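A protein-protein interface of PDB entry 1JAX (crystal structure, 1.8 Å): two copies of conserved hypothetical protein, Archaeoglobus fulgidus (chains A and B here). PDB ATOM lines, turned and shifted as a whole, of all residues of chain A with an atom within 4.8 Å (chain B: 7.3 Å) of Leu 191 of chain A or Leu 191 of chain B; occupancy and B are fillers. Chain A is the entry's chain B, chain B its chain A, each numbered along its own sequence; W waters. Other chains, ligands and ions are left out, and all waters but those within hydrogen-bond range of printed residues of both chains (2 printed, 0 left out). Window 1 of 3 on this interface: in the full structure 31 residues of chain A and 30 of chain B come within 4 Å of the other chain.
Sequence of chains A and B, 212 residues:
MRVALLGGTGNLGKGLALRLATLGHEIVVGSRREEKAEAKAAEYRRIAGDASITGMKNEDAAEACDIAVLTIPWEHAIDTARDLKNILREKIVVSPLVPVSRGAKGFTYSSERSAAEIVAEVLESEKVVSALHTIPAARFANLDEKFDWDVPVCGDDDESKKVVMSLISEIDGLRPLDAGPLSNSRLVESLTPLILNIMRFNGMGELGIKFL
N of Asp 150 of chain B lies within hydrogen-bond range of O of Ile 209 of chain B (2.8 Å). N of Phe 211 of chain B sits at hydrogen-bond distance from OD2 of Asp 150 of chain B, 2.8 Å away. OG of Ser 190 of chain B sits at hydrogen-bond distance from O of Arg 186 of chain B (2.6 Å). ND2 of Asn 197 of chain B sits at hydrogen-bond distance from O of Pro 193 of chain B.
Leu 187 of chain A touches Leu 194 of chain B, and with the chains exchanged Leu 194 of chain A touches Leu 187 of chain B. Leu 191 of chain A touches Leu 194 of chain B, and with the chains exchanged Leu 194 of chain A touches Leu 191 of chain B. Ile 195 of chain A touches Phe 211 of chain B, and with the chains exchanged Phe 211 of chain A touches Ile 195 of chain B. Ile 209 of chain A touches Phe 211 of chain B, and with the chains exchanged Phe 211 of chain A touches Ile 209 of chain B. Of the 15 pairs that touch across the chains among the printed residues, 11 have their exchanged pair printed and touching as well.
Water W2 bridges the backbone carbonyl oxygen (O) of Leu 187 of chain A (2.7 Å) and the backbone carbonyl oxygen (O) of Ser 190 of chain B (3.2 Å). Water W1 lies within hydrogen-bond range of the backbone carbonyl oxygen (O) of Leu 187 of chain B (2.7 Å) and the backbone carbonyl oxygen (O) of Ser 190 of chain A (3.4 Å).
Among the printed residues, pairs that only touch across the chains: Leu 191 of chain A with Leu 191 of chain B, Leu 187 of chain A with Asn 197 of chain B, Leu 194 of chain A with Leu 191 of chain B, Phe 211 of chain A with Ile 209 of chain B, Leu 191 of chain A with Leu 194 of chain B, Ile 195 of chain A with Phe 211 of chain B, Val 188 of chain A with Leu 194 of chain B, Leu 194 of chain A with Val 188 of chain B, Phe 211 of chain A with Ile 198 of chain B, Phe 211 of chain A with Ile 195 of chain B, Leu 194 of chain A with Leu 187 of chain B, Leu 187 of chain A with Leu 194 of chain B, Leu 187 of chain A with Ser 190 of chain B, Ile 209 of chain A with Phe 211 of chain B and Pro 193 of chain A with Leu 187 of chain B.
Leu 191 of chain A touches just these residues of chain B: Leu 191 (3.4 Å) and Leu 194 (3.7 Å). Of chain A, only Leu 191 (3.4 Å) and Leu 194 (3.7 Å) come within 4 Å of Leu 191 of chain B. Printed residues of chain A within 4 Å of Leu 194 of chain B: Leu 187 (3.9 Å), Val 188 (3.8 Å) and Leu 191 (3.7 Å). Of the printed residues of chain A, Val 188 of chain B touches Leu 194. Printed residues of chain B within 4 Å of Ile 195 of chain A: Phe 211. Of the printed residues of chain A, Leu 187 of chain B touches Pro 193 (3.99 Å) and Leu 194 (3.9 Å). Thr 192 of chain B touches none of the printed residues of chain A. The nearest printed residue of chain A that does not touch Leu 191 of chain B is Ile 209 of chain A (4.6 Å).
Of the 13 printed residues of chain A, 8 touch a printed residue of chain B. Hydrophobic or aromatic side chains of chain A that line the printed part of chain B: Leu 187, Val 188, Leu 191, Pro 193, Leu 194, Ile 195, Ile 209 and Phe 211. Hydrophobic or aromatic side chains of chain B within 4 Å of the printed part of chain A: Leu 187, Val 188, Leu 191, Leu 194, Ile 195, Ile 198, Ile 209 and Phe 211. Among the printed residues, 15 pairs touch across the chains.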
ATOM      1  N   THR A 134      35.252 -17.344 -15.649  1.00  0.00           N
ATOM      2  CA  THR A 134      34.112 -18.230 -15.431  1.00  0.00           C
ATOM      3  C   THR A 134      33.543 -18.861 -16.667  1.00  0.00           C
ATOM      4  O   THR A 134      32.332 -18.989 -16.801  1.00  0.00           O
ATOM      5  CB  THR A 134      32.952 -17.509 -14.724  1.00  0.00           C
ATOM      6  OG1 THR A 134      32.431 -16.474 -15.587  1.00  0.00           O
ATOM      7  CG2 THR A 134      33.419 -16.922 -13.419  1.00  0.00           C
ATOM      8  N   PRO A 152      32.454 -11.016 -16.893  1.00  0.00           N
ATOM      9  CA  PRO A 152      32.820  -9.741 -16.276  1.00  0.00           C
ATOM     10  C   PRO A 152      34.267  -9.424 -16.687  1.00  0.00           C
ATOM     11  O   PRO A 152      35.117 -10.306 -16.676  1.00  0.00           O
ATOM     12  CB  PRO A 152      32.723 -10.033 -14.782  1.00  0.00           C
ATOM     13  CG  PRO A 152      31.663 -11.151 -14.730  1.00  0.00           C
ATOM     14  CD  PRO A 152      32.053 -12.020 -15.874  1.00  0.00           C
ATOM     15  N   LEU A 187      36.773  -9.584  -6.949  1.00  0.00           N
ATOM     16  CA  LEU A 187      35.335  -9.906  -6.928  1.00  0.00           C
ATOM     17  C   LEU A 187      34.970 -10.775  -8.114  1.00  0.00           C
ATOM     18  O   LEU A 187      34.110 -11.649  -8.022  1.00  0.00           O
ATOM     19  CB  LEU A 187      34.496  -8.620  -6.967  1.00  0.00           C
ATOM     20  CG  LEU A 187      34.687  -7.733  -5.733  1.00  0.00           C
ATOM     21  CD1 LEU A 187      33.931  -6.411  -5.952  1.00  0.00           C
ATOM     22  CD2 LEU A 187      34.175  -8.453  -4.461  1.00  0.00           C
ATOM     23  N   VAL A 188      35.632 -10.528  -9.243  1.00  0.00           N
ATOM     24  CA  VAL A 188      35.346 -11.332 -10.425  1.00  0.00           C
ATOM     25  C   VAL A 188      35.992 -12.707 -10.281  1.00  0.00           C
ATOM     26  O   VAL A 188      35.372 -13.737 -10.576  1.00  0.00           O
ATOM     27  CB  VAL A 188      35.874 -10.645 -11.709  1.00  0.00           C
ATOM     28  CG1 VAL A 188      35.625 -11.558 -12.931  1.00  0.00           C
ATOM     29  CG2 VAL A 188      35.172  -9.283 -11.890  1.00  0.00           C
ATOM     30  N   GLU A 189      37.251 -12.736  -9.850  1.00  0.00           N
ATOM     31  CA  GLU A 189      37.950 -14.002  -9.701  1.00  0.00           C
ATOM     32  C   GLU A 189      37.277 -14.895  -8.677  1.00  0.00           C
ATOM     33  O   GLU A 189      37.313 -16.130  -8.796  1.00  0.00           O
ATOM     34  CB  GLU A 189      39.403 -13.740  -9.287  1.00  0.00           C
ATOM     35  CG  GLU A 189      40.230 -13.006 -10.372  1.00  0.00           C
ATOM     36  CD  GLU A 189      41.595 -12.562  -9.861  1.00  0.00           C
ATOM     37  OE1 GLU A 189      42.025 -13.059  -8.795  1.00  0.00           O
ATOM     38  OE2 GLU A 189      42.250 -11.716 -10.524  1.00  0.00           O
ATOM     39  N   SER A 190      36.658 -14.288  -7.673  1.00  0.00           N
ATOM     40  CA  SER A 190      35.999 -15.066  -6.618  1.00  0.00           C
ATOM     41  C   SER A 190      34.851 -15.919  -7.161  1.00  0.00           C
ATOM     42  O   SER A 190      34.472 -16.916  -6.552  1.00  0.00           O
ATOM     43  CB  SER A 190      35.461 -14.131  -5.535  1.00  0.00           C
ATOM     44  OG  SER A 190      36.520 -13.516  -4.837  1.00  0.00           O
ATOM     45  N   LEU A 191      34.299 -15.538  -8.302  1.00  0.00           N
ATOM     46  CA  LEU A 191      33.196 -16.309  -8.855  1.00  0.00           C
ATOM     47  C   LEU A 191      33.602 -17.762  -9.073  1.00  0.00           C
ATOM     48  O   LEU A 191      32.754 -18.658  -8.989  1.00  0.00           O
ATOM     49  CB  LEU A 191      32.755 -15.718 -10.188  1.00  0.00           C
ATOM     50  CG  LEU A 191      32.047 -14.371 -10.114  1.00  0.00           C
ATOM     51  CD1 LEU A 191      31.830 -13.846 -11.541  1.00  0.00           C
ATOM     52  CD2 LEU A 191      30.728 -14.522  -9.365  1.00  0.00           C
ATOM     53  N   THR A 192      34.887 -18.013  -9.349  1.00  0.00           N
ATOM     54  CA  THR A 192      35.326 -19.378  -9.597  1.00  0.00           C
ATOM     55  C   THR A 192      35.187 -20.273  -8.371  1.00  0.00           C
ATOM     56  O   THR A 192      34.518 -21.303  -8.444  1.00  0.00           O
ATOM     57  CB  THR A 192      36.772 -19.411 -10.153  1.00  0.00           C
ATOM     58  OG1 THR A 192      36.748 -18.864 -11.478  1.00  0.00           O
ATOM     59  CG2 THR A 192      37.297 -20.850 -10.233  1.00  0.00           C
ATOM     60  N   PRO A 193      35.798 -19.898  -7.232  1.00  0.00           N
ATOM     61  CA  PRO A 193      35.588 -20.822  -6.101  1.00  0.00           C
ATOM     62  C   PRO A 193      34.098 -20.879  -5.686  1.00  0.00           C
ATOM     63  O   PRO A 193      33.626 -21.887  -5.142  1.00  0.00           O
ATOM     64  CB  PRO A 193      36.517 -20.265  -5.000  1.00  0.00           C
ATOM     65  CG  PRO A 193      36.779 -18.784  -5.432  1.00  0.00           C
ATOM     66  CD  PRO A 193      36.827 -18.878  -6.939  1.00  0.00           C
ATOM     67  N   LEU A 194      33.344 -19.802  -5.899  1.00  0.00           N
ATOM     68  CA  LEU A 194      31.908 -19.892  -5.569  1.00  0.00           C
ATOM     69  C   LEU A 194      31.281 -20.979  -6.431  1.00  0.00           C
ATOM     70  O   LEU A 194      30.572 -21.868  -5.933  1.00  0.00           O
ATOM     71  CB  LEU A 194      31.198 -18.571  -5.862  1.00  0.00           C
ATOM     72  CG  LEU A 194      29.668 -18.586  -5.772  1.00  0.00           C
ATOM     73  CD1 LEU A 194      29.249 -18.993  -4.376  1.00  0.00           C
ATOM     74  CD2 LEU A 194      29.132 -17.194  -6.066  1.00  0.00           C
ATOM     75  N   ILE A 195      31.513 -20.895  -7.741  1.00  0.00           N
ATOM     76  CA  ILE A 195      30.933 -21.883  -8.652  1.00  0.00           C
ATOM     77  C   ILE A 195      31.415 -23.308  -8.343  1.00  0.00           C
ATOM     78  O   ILE A 195      30.609 -24.236  -8.371  1.00  0.00           O
ATOM     79  CB  ILE A 195      31.230 -21.505 -10.129  1.00  0.00           C
ATOM     80  CG1 ILE A 195      30.420 -20.256 -10.485  1.00  0.00           C
ATOM     81  CG2 ILE A 195      30.898 -22.679 -11.073  1.00  0.00           C
ATOM     82  CD1 ILE A 195      30.866 -19.571 -11.766  1.00  0.00           C
ATOM     83  N   ILE A 209      27.886 -18.178 -15.564  1.00  0.00           N
ATOM     84  CA  ILE A 209      26.991 -17.295 -14.825  1.00  0.00           C
ATOM     85  C   ILE A 209      26.325 -16.276 -15.766  1.00  0.00           C
ATOM     86  O   ILE A 209      26.881 -15.931 -16.814  1.00  0.00           O
ATOM     87  CB  ILE A 209      27.788 -16.557 -13.704  1.00  0.00           C
ATOM     88  CG1 ILE A 209      26.828 -15.916 -12.697  1.00  0.00           C
ATOM     89  CG2 ILE A 209      28.692 -15.488 -14.326  1.00  0.00           C
ATOM     90  CD1 ILE A 209      27.509 -15.505 -11.398  1.00  0.00           C
ATOM     91  N   PHE A 211      23.932 -12.553 -15.499  1.00  0.00           N
ATOM     92  CA  PHE A 211      23.390 -11.505 -14.632  1.00  0.00           C
ATOM     93  C   PHE A 211      22.141 -11.003 -15.340  1.00  0.00           C
ATOM     94  O   PHE A 211      22.205 -10.534 -16.470  1.00  0.00           O
ATOM     95  CB  PHE A 211      24.421 -10.388 -14.455  1.00  0.00           C
ATOM     96  CG  PHE A 211      25.670 -10.848 -13.774  1.00  0.00           C
ATOM     97  CD1 PHE A 211      26.762 -11.301 -14.505  1.00  0.00           C
ATOM     98  CD2 PHE A 211      25.736 -10.880 -12.376  1.00  0.00           C
ATOM     99  CE1 PHE A 211      27.911 -11.779 -13.851  1.00  0.00           C
ATOM    100  CE2 PHE A 211      26.874 -11.355 -11.724  1.00  0.00           C
ATOM    101  CZ  PHE A 211      27.962 -11.802 -12.464  1.00  0.00           C
ATOM    102  N   VAL B  98      25.400  -7.979   3.726  1.00  0.00           N
ATOM    103  CA  VAL B  98      26.656  -7.911   2.988  1.00  0.00           C
ATOM    104  C   VAL B  98      27.382  -6.636   3.401  1.00  0.00           C
ATOM    105  O   VAL B  98      26.779  -5.577   3.432  1.00  0.00           O
ATOM    106  CB  VAL B  98      26.430  -7.780   1.462  1.00  0.00           C
ATOM    107  CG1 VAL B  98      27.763  -7.654   0.757  1.00  0.00           C
ATOM    108  CG2 VAL B  98      25.659  -8.967   0.910  1.00  0.00           C
ATOM    109  N   TYR B 109      34.167  -5.286  -1.043  1.00  0.00           N
ATOM    110  CA  TYR B 109      33.747  -6.100   0.081  1.00  0.00           C
ATOM    111  C   TYR B 109      34.538  -5.496   1.240  1.00  0.00           C
ATOM    112  O   TYR B 109      35.775  -5.537   1.261  1.00  0.00           O
ATOM    113  CB  TYR B 109      34.156  -7.532  -0.170  1.00  0.00           C
ATOM    114  CG  TYR B 109      33.521  -8.471   0.808  1.00  0.00           C
ATOM    115  CD1 TYR B 109      32.177  -8.816   0.682  1.00  0.00           C
ATOM    116  CD2 TYR B 109      34.242  -8.968   1.877  1.00  0.00           C
ATOM    117  CE1 TYR B 109      31.563  -9.642   1.616  1.00  0.00           C
ATOM    118  CE2 TYR B 109      33.647  -9.797   2.813  1.00  0.00           C
ATOM    119  CZ  TYR B 109      32.307 -10.130   2.669  1.00  0.00           C
ATOM    120  OH  TYR B 109      31.727 -10.997   3.557  1.00  0.00           O
ATOM    121  N   HIS B 133      21.148 -12.749  -0.493  1.00  0.00           N
ATOM    122  CA  HIS B 133      21.925 -11.522  -0.692  1.00  0.00           C
ATOM    123  C   HIS B 133      21.749 -10.898  -2.067  1.00  0.00           C
ATOM    124  O   HIS B 133      21.869  -9.684  -2.217  1.00  0.00           O
ATOM    125  CB  HIS B 133      23.422 -11.812  -0.554  1.00  0.00           C
ATOM    126  CG  HIS B 133      23.754 -12.754   0.561  1.00  0.00           C
ATOM    127  ND1 HIS B 133      23.584 -14.119   0.451  1.00  0.00           N
ATOM    128  CD2 HIS B 133      24.253 -12.533   1.802  1.00  0.00           C
ATOM    129  CE1 HIS B 133      23.972 -14.699   1.574  1.00  0.00           C
ATOM    130  NE2 HIS B 133      24.381 -13.761   2.412  1.00  0.00           N
ATOM    131  N   THR B 134      21.511 -11.719  -3.080  1.00  0.00           N
ATOM    132  CA  THR B 134      21.450 -11.179  -4.437  1.00  0.00           C
ATOM    133  C   THR B 134      20.077 -11.118  -5.053  1.00  0.00           C
ATOM    134  O   THR B 134      19.886 -11.466  -6.227  1.00  0.00           O
ATOM    135  CB  THR B 134      22.366 -11.965  -5.391  1.00  0.00           C
ATOM    136  OG1 THR B 134      21.844 -13.287  -5.569  1.00  0.00           O
ATOM    137  CG2 THR B 134      23.761 -12.081  -4.798  1.00  0.00           C
ATOM    138  N   ASP B 150      19.076 -17.703  -9.107  1.00  0.00           N
ATOM    139  CA  ASP B 150      19.569 -18.738  -8.220  1.00  0.00           C
ATOM    140  C   ASP B 150      19.974 -18.047  -6.925  1.00  0.00           C
ATOM    141  O   ASP B 150      20.416 -16.880  -6.917  1.00  0.00           O
ATOM    142  CB  ASP B 150      20.784 -19.496  -8.792  1.00  0.00           C
ATOM    143  CG  ASP B 150      20.409 -20.416  -9.933  1.00  0.00           C
ATOM    144  OD1 ASP B 150      19.214 -20.795 -10.018  1.00  0.00           O
ATOM    145  OD2 ASP B 150      21.311 -20.785 -10.725  1.00  0.00           O
ATOM    146  N   VAL B 151      19.846 -18.786  -5.830  1.00  0.00           N
ATOM    147  CA  VAL B 151      20.152 -18.251  -4.513  1.00  0.00           C
ATOM    148  C   VAL B 151      21.119 -19.159  -3.771  1.00  0.00           C
ATOM    149  O   VAL B 151      20.717 -20.186  -3.241  1.00  0.00           O
ATOM    150  CB  VAL B 151      18.866 -18.156  -3.642  1.00  0.00           C
ATOM    151  CG1 VAL B 151      19.200 -17.521  -2.280  1.00  0.00           C
ATOM    152  CG2 VAL B 151      17.787 -17.392  -4.373  1.00  0.00           C
ATOM    153  N   PRO B 152      22.416 -18.798  -3.744  1.00  0.00           N
ATOM    154  CA  PRO B 152      23.388 -19.635  -3.027  1.00  0.00           C
ATOM    155  C   PRO B 152      23.070 -19.576  -1.517  1.00  0.00           C
ATOM    156  O   PRO B 152      22.772 -18.500  -0.971  1.00  0.00           O
ATOM    157  CB  PRO B 152      24.729 -18.981  -3.363  1.00  0.00           C
ATOM    158  CG  PRO B 152      24.463 -18.368  -4.771  1.00  0.00           C
ATOM    159  CD  PRO B 152      23.089 -17.741  -4.528  1.00  0.00           C
ATOM    160  N   SER B 185      30.499 -18.139   3.135  1.00  0.00           N
ATOM    161  CA  SER B 185      29.591 -17.008   3.022  1.00  0.00           C
ATOM    162  C   SER B 185      30.243 -15.791   2.374  1.00  0.00           C
ATOM    163  O   SER B 185      29.569 -15.049   1.656  1.00  0.00           O
ATOM    164  CB  SER B 185      28.992 -16.627   4.389  1.00  0.00           C
ATOM    165  OG  SER B 185      27.876 -15.756   4.204  1.00  0.00           O
ATOM    166  N   ARG B 186      31.548 -15.606   2.576  1.00  0.00           N
ATOM    167  CA  ARG B 186      32.184 -14.442   1.960  1.00  0.00           C
ATOM    168  C   ARG B 186      32.062 -14.495   0.440  1.00  0.00           C
ATOM    169  O   ARG B 186      31.897 -13.458  -0.220  1.00  0.00           O
ATOM    170  CB  ARG B 186      33.670 -14.333   2.337  1.00  0.00           C
ATOM    171  CG  ARG B 186      34.372 -13.188   1.571  1.00  0.00           C
ATOM    172  CD  ARG B 186      35.770 -12.856   2.095  1.00  0.00           C
ATOM    173  NE  ARG B 186      36.350 -11.743   1.342  1.00  0.00           N
ATOM    174  CZ  ARG B 186      37.380 -11.013   1.763  1.00  0.00           C
ATOM    175  NH1 ARG B 186      37.950 -11.280   2.930  1.00  0.00           N
ATOM    176  NH2 ARG B 186      37.833 -10.008   1.024  1.00  0.00           N
ATOM    177  N   LEU B 187      32.143 -15.696  -0.127  1.00  0.00           N
ATOM    178  CA  LEU B 187      32.077 -15.856  -1.588  1.00  0.00           C
ATOM    179  C   LEU B 187      30.682 -15.513  -2.092  1.00  0.00           C
ATOM    180  O   LEU B 187      30.501 -14.988  -3.194  1.00  0.00           O
ATOM    181  CB  LEU B 187      32.415 -17.302  -1.998  1.00  0.00           C
ATOM    182  CG  LEU B 187      33.838 -17.774  -1.653  1.00  0.00           C
ATOM    183  CD1 LEU B 187      33.964 -19.254  -1.951  1.00  0.00           C
ATOM    184  CD2 LEU B 187      34.866 -16.962  -2.447  1.00  0.00           C
ATOM    185  N   VAL B 188      29.685 -15.830  -1.291  1.00  0.00           N
ATOM    186  CA  VAL B 188      28.322 -15.514  -1.693  1.00  0.00           C
ATOM    187  C   VAL B 188      28.008 -14.037  -1.501  1.00  0.00           C
ATOM    188  O   VAL B 188      27.410 -13.404  -2.366  1.00  0.00           O
ATOM    189  CB  VAL B 188      27.309 -16.346  -0.900  1.00  0.00           C
ATOM    190  CG1 VAL B 188      25.880 -15.919  -1.273  1.00  0.00           C
ATOM    191  CG2 VAL B 188      27.526 -17.798  -1.197  1.00  0.00           C
ATOM    192  N   GLU B 189      28.393 -13.492  -0.351  1.00  0.00           N
ATOM    193  CA  GLU B 189      28.158 -12.083  -0.061  1.00  0.00           C
ATOM    194  C   GLU B 189      28.876 -11.184  -1.069  1.00  0.00           C
ATOM    195  O   GLU B 189      28.378 -10.103  -1.413  1.00  0.00           O
ATOM    196  CB  GLU B 189      28.621 -11.758   1.368  1.00  0.00           C
ATOM    197  CG  GLU B 189      27.771 -12.458   2.453  1.00  0.00           C
ATOM    198  CD  GLU B 189      28.349 -12.267   3.859  1.00  0.00           C
ATOM    199  OE1 GLU B 189      29.137 -11.307   4.067  1.00  0.00           O
ATOM    200  OE2 GLU B 189      28.009 -13.073   4.765  1.00  0.00           O
ATOM    201  N   SER B 190      30.017 -11.656  -1.574  1.00  0.00           N
ATOM    202  CA  SER B 190      30.816 -10.891  -2.534  1.00  0.00           C
ATOM    203  C   SER B 190      30.091 -10.647  -3.861  1.00  0.00           C
ATOM    204  O   SER B 190      30.464  -9.755  -4.640  1.00  0.00           O
ATOM    205  CB  SER B 190      32.154 -11.603  -2.772  1.00  0.00           C
ATOM    206  OG  SER B 190      32.947 -11.485  -1.590  1.00  0.00           O
ATOM    207  N   LEU B 191      29.078 -11.455  -4.148  1.00  0.00           N
ATOM    208  CA  LEU B 191      28.307 -11.224  -5.381  1.00  0.00           C
ATOM    209  C   LEU B 191      27.652  -9.821  -5.376  1.00  0.00           C
ATOM    210  O   LEU B 191      27.490  -9.200  -6.415  1.00  0.00           O
ATOM    211  CB  LEU B 191      27.195 -12.251  -5.512  1.00  0.00           C
ATOM    212  CG  LEU B 191      27.659 -13.688  -5.749  1.00  0.00           C
ATOM    213  CD1 LEU B 191      26.453 -14.624  -5.579  1.00  0.00           C
ATOM    214  CD2 LEU B 191      28.252 -13.820  -7.147  1.00  0.00           C
ATOM    215  N   THR B 192      27.255  -9.325  -4.211  1.00  0.00           N
ATOM    216  CA  THR B 192      26.611  -8.021  -4.182  1.00  0.00           C
ATOM    217  C   THR B 192      27.495  -6.878  -4.681  1.00  0.00           C
ATOM    218  O   THR B 192      27.096  -6.136  -5.593  1.00  0.00           O
ATOM    219  CB  THR B 192      26.025  -7.740  -2.783  1.00  0.00           C
ATOM    220  OG1 THR B 192      24.932  -8.642  -2.582  1.00  0.00           O
ATOM    221  CG2 THR B 192      25.512  -6.309  -2.670  1.00  0.00           C
ATOM    222  N   PRO B 193      28.699  -6.707  -4.107  1.00  0.00           N
ATOM    223  CA  PRO B 193      29.495  -5.599  -4.652  1.00  0.00           C
ATOM    224  C   PRO B 193      29.877  -5.854  -6.116  1.00  0.00           C
ATOM    225  O   PRO B 193      30.089  -4.914  -6.883  1.00  0.00           O
ATOM    226  CB  PRO B 193      30.718  -5.531  -3.713  1.00  0.00           C
ATOM    227  CG  PRO B 193      30.726  -6.860  -2.991  1.00  0.00           C
ATOM    228  CD  PRO B 193      29.252  -7.171  -2.824  1.00  0.00           C
ATOM    229  N   LEU B 194      29.991  -7.118  -6.513  1.00  0.00           N
ATOM    230  CA  LEU B 194      30.330  -7.380  -7.916  1.00  0.00           C
ATOM    231  C   LEU B 194      29.179  -6.855  -8.796  1.00  0.00           C
ATOM    232  O   LEU B 194      29.380  -6.172  -9.795  1.00  0.00           O
ATOM    233  CB  LEU B 194      30.508  -8.888  -8.154  1.00  0.00           C
ATOM    234  CG  LEU B 194      30.567  -9.298  -9.641  1.00  0.00           C
ATOM    235  CD1 LEU B 194      31.763  -8.613 -10.343  1.00  0.00           C
ATOM    236  CD2 LEU B 194      30.730 -10.832  -9.728  1.00  0.00           C
ATOM    237  N   ILE B 195      27.960  -7.198  -8.417  1.00  0.00           N
ATOM    238  CA  ILE B 195      26.807  -6.772  -9.184  1.00  0.00           C
ATOM    239  C   ILE B 195      26.684  -5.242  -9.167  1.00  0.00           C
ATOM    240  O   ILE B 195      26.403  -4.635 -10.206  1.00  0.00           O
ATOM    241  CB  ILE B 195      25.545  -7.457  -8.646  1.00  0.00           C
ATOM    242  CG1 ILE B 195      25.585  -8.943  -9.029  1.00  0.00           C
ATOM    243  CG2 ILE B 195      24.299  -6.782  -9.202  1.00  0.00           C
ATOM    244  CD1 ILE B 195      24.628  -9.823  -8.236  1.00  0.00           C
ATOM    245  N   LEU B 196      26.914  -4.621  -8.008  1.00  0.00           N
ATOM    246  CA  LEU B 196      26.838  -3.162  -7.944  1.00  0.00           C
ATOM    247  C   LEU B 196      27.875  -2.550  -8.906  1.00  0.00           C
ATOM    248  O   LEU B 196      27.633  -1.485  -9.509  1.00  0.00           O
ATOM    249  CB  LEU B 196      27.058  -2.686  -6.501  1.00  0.00           C
ATOM    250  CG  LEU B 196      25.905  -3.101  -5.552  1.00  0.00           C
ATOM    251  CD1 LEU B 196      26.269  -2.779  -4.108  1.00  0.00           C
ATOM    252  CD2 LEU B 196      24.612  -2.363  -5.923  1.00  0.00           C
ATOM    253  N   ASN B 197      29.037  -3.197  -9.058  1.00  0.00           N
ATOM    254  CA  ASN B 197      30.024  -2.677 -10.008  1.00  0.00           C
ATOM    255  C   ASN B 197      29.513  -2.842 -11.432  1.00  0.00           C
ATOM    256  O   ASN B 197      29.618  -1.921 -12.249  1.00  0.00           O
ATOM    257  CB  ASN B 197      31.394  -3.372  -9.874  1.00  0.00           C
ATOM    258  CG  ASN B 197      32.179  -2.864  -8.677  1.00  0.00           C
ATOM    259  OD1 ASN B 197      32.310  -1.652  -8.491  1.00  0.00           O
ATOM    260  ND2 ASN B 197      32.702  -3.774  -7.862  1.00  0.00           N
ATOM    261  N   ILE B 198      28.959  -4.012 -11.734  1.00  0.00           N
ATOM    262  CA  ILE B 198      28.432  -4.260 -13.073  1.00  0.00           C
ATOM    263  C   ILE B 198      27.343  -3.245 -13.405  1.00  0.00           C
ATOM    264  O   ILE B 198      27.302  -2.714 -14.520  1.00  0.00           O
ATOM    265  CB  ILE B 198      27.892  -5.695 -13.170  1.00  0.00           C
ATOM    266  CG1 ILE B 198      29.082  -6.653 -13.153  1.00  0.00           C
ATOM    267  CG2 ILE B 198      27.086  -5.891 -14.467  1.00  0.00           C
ATOM    268  CD1 ILE B 198      28.695  -8.097 -13.014  1.00  0.00           C
ATOM    269  N   LEU B 207      20.255  -6.347 -10.772  1.00  0.00           N
ATOM    270  CA  LEU B 207      20.321  -7.691 -11.339  1.00  0.00           C
ATOM    271  C   LEU B 207      20.481  -8.769 -10.295  1.00  0.00           C
ATOM    272  O   LEU B 207      20.965  -8.519  -9.194  1.00  0.00           O
ATOM    273  CB  LEU B 207      21.559  -7.774 -12.243  1.00  0.00           C
ATOM    274  CG  LEU B 207      21.728  -6.626 -13.237  1.00  0.00           C
ATOM    275  CD1 LEU B 207      23.152  -6.606 -13.808  1.00  0.00           C
ATOM    276  CD2 LEU B 207      20.683  -6.800 -14.323  1.00  0.00           C
ATOM    277  N   ILE B 209      21.470 -13.242 -10.127  1.00  0.00           N
ATOM    278  CA  ILE B 209      22.412 -14.148 -10.752  1.00  0.00           C
ATOM    279  C   ILE B 209      21.768 -15.490 -11.058  1.00  0.00           C
ATOM    280  O   ILE B 209      20.808 -15.896 -10.405  1.00  0.00           O
ATOM    281  CB  ILE B 209      23.610 -14.404  -9.844  1.00  0.00           C
ATOM    282  CG1 ILE B 209      23.107 -14.942  -8.499  1.00  0.00           C
ATOM    283  CG2 ILE B 209      24.412 -13.112  -9.673  1.00  0.00           C
ATOM    284  CD1 ILE B 209      24.142 -15.687  -7.702  1.00  0.00           C
ATOM    285  N   PHE B 211      23.129 -19.545 -12.475  1.00  0.00           N
ATOM    286  CA  PHE B 211      24.221 -20.418 -12.921  1.00  0.00           C
ATOM    287  C   PHE B 211      23.674 -21.319 -14.017  1.00  0.00           C
ATOM    288  O   PHE B 211      22.630 -21.960 -13.836  1.00  0.00           O
ATOM    289  CB  PHE B 211      24.735 -21.243 -11.743  1.00  0.00           C
ATOM    290  CG  PHE B 211      25.233 -20.389 -10.617  1.00  0.00           C
ATOM    291  CD1 PHE B 211      24.383 -20.018  -9.575  1.00  0.00           C
ATOM    292  CD2 PHE B 211      26.530 -19.887 -10.643  1.00  0.00           C
ATOM    293  CE1 PHE B 211      24.820 -19.153  -8.569  1.00  0.00           C
ATOM    294  CE2 PHE B 211      26.985 -19.020  -9.645  1.00  0.00           C
ATOM    295  CZ  PHE B 211      26.130 -18.650  -8.603  1.00  0.00           C
HETATM  296  O   HOH W   1      32.117 -14.736  -5.404  1.00  0.00           O
HETATM  297  O   HOH W   2      31.959 -12.037  -6.371  1.00  0.00           O
